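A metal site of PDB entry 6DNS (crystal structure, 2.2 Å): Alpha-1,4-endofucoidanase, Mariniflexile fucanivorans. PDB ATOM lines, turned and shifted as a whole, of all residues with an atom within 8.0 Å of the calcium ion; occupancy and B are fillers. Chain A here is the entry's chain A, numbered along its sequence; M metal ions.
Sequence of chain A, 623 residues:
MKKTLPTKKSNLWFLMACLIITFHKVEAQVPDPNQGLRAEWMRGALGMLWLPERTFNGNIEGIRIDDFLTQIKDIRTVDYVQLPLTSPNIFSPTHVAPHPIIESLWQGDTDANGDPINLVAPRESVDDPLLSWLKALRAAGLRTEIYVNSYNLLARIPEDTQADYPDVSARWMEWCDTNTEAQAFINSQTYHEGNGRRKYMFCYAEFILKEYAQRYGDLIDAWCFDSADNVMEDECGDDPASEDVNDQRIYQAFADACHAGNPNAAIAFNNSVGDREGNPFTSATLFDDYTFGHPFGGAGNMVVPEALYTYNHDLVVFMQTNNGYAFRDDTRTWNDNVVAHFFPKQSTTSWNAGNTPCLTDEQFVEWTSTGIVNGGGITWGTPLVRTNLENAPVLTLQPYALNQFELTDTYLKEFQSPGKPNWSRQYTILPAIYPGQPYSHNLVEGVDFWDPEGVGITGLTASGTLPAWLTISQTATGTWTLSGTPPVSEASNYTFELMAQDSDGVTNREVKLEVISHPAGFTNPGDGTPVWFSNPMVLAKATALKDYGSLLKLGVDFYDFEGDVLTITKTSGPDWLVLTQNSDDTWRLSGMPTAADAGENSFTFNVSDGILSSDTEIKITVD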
ATOM      1  N   ALA A 326      -2.428 -23.587  13.475  1.00  0.00           N
ATOM      2  CA  ALA A 326      -2.200 -24.569  14.538  1.00  0.00           C
ATOM      3  C   ALA A 326      -0.933 -25.401  14.368  1.00  0.00           C
ATOM      4  O   ALA A 326      -0.215 -25.642  15.344  1.00  0.00           O
ATOM      5  CB  ALA A 326      -3.411 -25.496  14.664  1.00  0.00           C
ATOM      6  N   PHE A 327      -0.656 -25.826  13.139  1.00  0.00           N
ATOM      7  CA  PHE A 327       0.373 -26.843  12.880  1.00  0.00           C
ATOM      8  C   PHE A 327       1.442 -26.368  11.886  1.00  0.00           C
ATOM      9  O   PHE A 327       1.757 -27.053  10.918  1.00  0.00           O
ATOM     10  CB  PHE A 327      -0.289 -28.140  12.406  1.00  0.00           C
ATOM     11  CG  PHE A 327      -1.384 -28.616  13.326  1.00  0.00           C
ATOM     12  CD1 PHE A 327      -1.088 -29.039  14.619  1.00  0.00           C
ATOM     13  CD2 PHE A 327      -2.718 -28.617  12.908  1.00  0.00           C
ATOM     14  CE1 PHE A 327      -2.085 -29.463  15.482  1.00  0.00           C
ATOM     15  CE2 PHE A 327      -3.722 -29.047  13.769  1.00  0.00           C
ATOM     16  CZ  PHE A 327      -3.413 -29.468  15.056  1.00  0.00           C
ATOM     17  N   ARG A 328       2.003 -25.193  12.167  1.00  0.00           N
ATOM     18  CA  ARG A 328       3.138 -24.657  11.406  1.00  0.00           C
ATOM     19  C   ARG A 328       4.462 -25.279  11.900  1.00  0.00           C
ATOM     20  O   ARG A 328       5.442 -25.332  11.169  1.00  0.00           O
ATOM     21  CB  ARG A 328       3.190 -23.128  11.547  1.00  0.00           C
ATOM     22  CG  ARG A 328       3.449 -22.356  10.254  1.00  0.00           C
ATOM     23  CD  ARG A 328       2.188 -22.115   9.432  1.00  0.00           C
ATOM     24  NE  ARG A 328       2.239 -20.844   8.689  1.00  0.00           N
ATOM     25  CZ  ARG A 328       1.271 -20.378   7.901  1.00  0.00           C
ATOM     26  NH1 ARG A 328       0.147 -21.062   7.691  1.00  0.00           N
ATOM     27  NH2 ARG A 328       1.435 -19.199   7.286  1.00  0.00           N
ATOM     28  N   ASP A 329       4.457 -25.753  13.154  1.00  0.00           N
ATOM     29  CA  ASP A 329       5.646 -26.292  13.831  1.00  0.00           C
ATOM     30  C   ASP A 329       6.142 -27.668  13.345  1.00  0.00           C
ATOM     31  O   ASP A 329       7.356 -27.895  13.315  1.00  0.00           O
ATOM     32  CB  ASP A 329       5.419 -26.346  15.354  1.00  0.00           C
ATOM     33  CG  ASP A 329       4.266 -27.287  15.756  1.00  0.00           C
ATOM     34  OD1 ASP A 329       3.234 -27.311  15.060  1.00  0.00           O
ATOM     35  OD2 ASP A 329       4.406 -27.995  16.776  1.00  0.00           O
ATOM     36  N   ASP A 330       5.221 -28.566  13.000  1.00  0.00           N
ATOM     37  CA  ASP A 330       5.558 -29.979  12.754  1.00  0.00           C
ATOM     38  C   ASP A 330       6.301 -30.237  11.432  1.00  0.00           C
ATOM     39  O   ASP A 330       6.603 -29.292  10.689  1.00  0.00           O
ATOM     40  CB  ASP A 330       4.300 -30.874  12.909  1.00  0.00           C
ATOM     41  CG  ASP A 330       3.222 -30.593  11.850  1.00  0.00           C
ATOM     42  OD1 ASP A 330       3.496 -29.950  10.815  1.00  0.00           O
ATOM     43  OD2 ASP A 330       2.065 -31.026  12.070  1.00  0.00           O
ATOM     44  N   THR A 331       6.578 -31.512  11.125  1.00  0.00           N
ATOM     45  CA  THR A 331       7.255 -31.909   9.883  1.00  0.00           C
ATOM     46  C   THR A 331       6.281 -32.256   8.736  1.00  0.00           C
ATOM     47  O   THR A 331       6.563 -33.129   7.916  1.00  0.00           O
ATOM     48  CB  THR A 331       8.200 -33.103  10.133  1.00  0.00           C
ATOM     49  OG1 THR A 331       7.432 -34.274  10.449  1.00  0.00           O
ATOM     50  CG2 THR A 331       9.168 -32.808  11.266  1.00  0.00           C
ATOM     51  N   ARG A 332       5.135 -31.555   8.673  1.00  0.00           N
ATOM     52  CA  ARG A 332       4.114 -31.767   7.644  1.00  0.00           C
ATOM     53  C   ARG A 332       3.691 -30.424   7.061  1.00  0.00           C
ATOM     54  O   ARG A 332       3.101 -29.607   7.771  1.00  0.00           O
ATOM     55  CB  ARG A 332       2.895 -32.478   8.243  1.00  0.00           C
ATOM     56  CG  ARG A 332       3.154 -33.874   8.792  1.00  0.00           C
ATOM     57  CD  ARG A 332       1.912 -34.399   9.495  1.00  0.00           C
ATOM     58  NE  ARG A 332       2.024 -35.799   9.910  1.00  0.00           N
ATOM     59  CZ  ARG A 332       1.067 -36.503  10.517  1.00  0.00           C
ATOM     60  NH1 ARG A 332      -0.118 -35.953  10.813  1.00  0.00           N
ATOM     61  NH2 ARG A 332       1.291 -37.770  10.849  1.00  0.00           N
ATOM     62  N   THR A 333       4.003 -30.168   5.795  1.00  0.00           N
ATOM     63  CA  THR A 333       3.622 -28.917   5.135  1.00  0.00           C
ATOM     64  C   THR A 333       2.144 -28.877   4.708  1.00  0.00           C
ATOM     65  O   THR A 333       1.576 -27.794   4.571  1.00  0.00           O
ATOM     66  CB  THR A 333       4.511 -28.618   3.907  1.00  0.00           C
ATOM     67  OG1 THR A 333       4.351 -29.646   2.926  1.00  0.00           O
ATOM     68  CG2 THR A 333       5.978 -28.506   4.313  1.00  0.00           C
ATOM     69  N   TRP A 334       1.544 -30.050   4.481  1.00  0.00           N
ATOM     70  CA  TRP A 334       0.142 -30.140   4.054  1.00  0.00           C
ATOM     71  C   TRP A 334      -0.895 -29.614   5.074  1.00  0.00           C
ATOM     72  O   TRP A 334      -2.001 -29.237   4.672  1.00  0.00           O
ATOM     73  CB  TRP A 334      -0.234 -31.562   3.591  1.00  0.00           C
ATOM     74  CG  TRP A 334      -0.106 -32.653   4.633  1.00  0.00           C
ATOM     75  CD1 TRP A 334       0.936 -33.527   4.783  1.00  0.00           C
ATOM     76  CD2 TRP A 334      -1.073 -33.016   5.633  1.00  0.00           C
ATOM     77  NE1 TRP A 334       0.695 -34.389   5.826  1.00  0.00           N
ATOM     78  CE2 TRP A 334      -0.529 -34.102   6.368  1.00  0.00           C
ATOM     79  CE3 TRP A 334      -2.328 -32.522   5.996  1.00  0.00           C
ATOM     80  CZ2 TRP A 334      -1.215 -34.699   7.431  1.00  0.00           C
ATOM     81  CZ3 TRP A 334      -3.014 -33.120   7.058  1.00  0.00           C
ATOM     82  CH2 TRP A 334      -2.444 -34.200   7.767  1.00  0.00           C
ATOM     83  N   ASN A 335      -0.530 -29.583   6.356  1.00  0.00           N
ATOM     84  CA  ASN A 335      -1.411 -29.041   7.412  1.00  0.00           C
ATOM     85  C   ASN A 335      -1.090 -27.602   7.865  1.00  0.00           C
ATOM     86  O   ASN A 335      -1.595 -27.158   8.899  1.00  0.00           O
ATOM     87  CB  ASN A 335      -1.455 -30.006   8.624  1.00  0.00           C
ATOM     88  CG  ASN A 335      -0.139 -30.099   9.381  1.00  0.00           C
ATOM     89  OD1 ASN A 335       0.734 -29.250   9.260  1.00  0.00           O
ATOM     90  ND2 ASN A 335       0.000 -31.153  10.171  1.00  0.00           N
ATOM     91  N   ASP A 336      -0.268 -26.882   7.091  1.00  0.00           N
ATOM     92  CA  ASP A 336       0.165 -25.520   7.453  1.00  0.00           C
ATOM     93  C   ASP A 336      -0.934 -24.460   7.369  1.00  0.00           C
ATOM     94  O   ASP A 336      -0.853 -23.438   8.071  1.00  0.00           O
ATOM     95  CB  ASP A 336       1.368 -25.072   6.603  1.00  0.00           C
ATOM     96  CG  ASP A 336       2.659 -25.795   6.954  1.00  0.00           C
ATOM     97  OD1 ASP A 336       2.663 -26.622   7.893  1.00  0.00           O
ATOM     98  OD2 ASP A 336       3.684 -25.533   6.283  1.00  0.00           O
ATOM     99  N   ASN A 337      -1.930 -24.676   6.527  1.00  0.00           N
ATOM    100  CA  ASN A 337      -3.072 -23.760   6.416  1.00  0.00           C
ATOM    101  C   ASN A 337      -4.222 -24.039   7.410  1.00  0.00           C
ATOM    102  O   ASN A 337      -5.188 -23.274   7.455  1.00  0.00           O
ATOM    103  CB  ASN A 337      -3.620 -23.750   4.972  1.00  0.00           C
ATOM    104  CG  ASN A 337      -2.664 -23.092   3.989  1.00  0.00           C
ATOM    105  OD1 ASN A 337      -1.975 -22.128   4.315  1.00  0.00           O
ATOM    106  ND2 ASN A 337      -2.633 -23.607   2.772  1.00  0.00           N
HETATM  107 CA    CA M   1       3.556 -27.986   9.576  1.00  0.00          CA
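The backbone carbonyl oxygen (O) of Phe 327 lies close to the side-chain amide oxygen (OD1) of Asn 335 (2.9 Å).
The side-chain amide nitrogen of Asn 335 sits at hydrogen-bond distance from the side-chain carboxylate of Asp 330.
The guanidinium group (NH1) of Arg 328 sits at hydrogen-bond distance from the backbone carbonyl oxygen (O) of Asp 336.
O of Arg 332 lies close to OD1 of Asn 335 (2.8 Å).
O of Arg 328 touches the calcium ion, at 3.6 Å.
Six residues have an atom within 4 Å of the calcium ion: Phe 327, Arg 328, Asp 330, Arg 332, Asn 335 and Asp 336.
The nearest printed residue that does not touch the calcium ion is Asp 329 (4.3 Å).
The calcium ion is bound by OD1 of Asp 330 (2.3 Å), OD1 of Asp 336 (2.3 Å), O of Phe 327 (2.4 Å) and O of Arg 332 (2.5 Å).
Slightly farther from the calcium ion lies OD1 of Asn 335 (3.1 Å).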
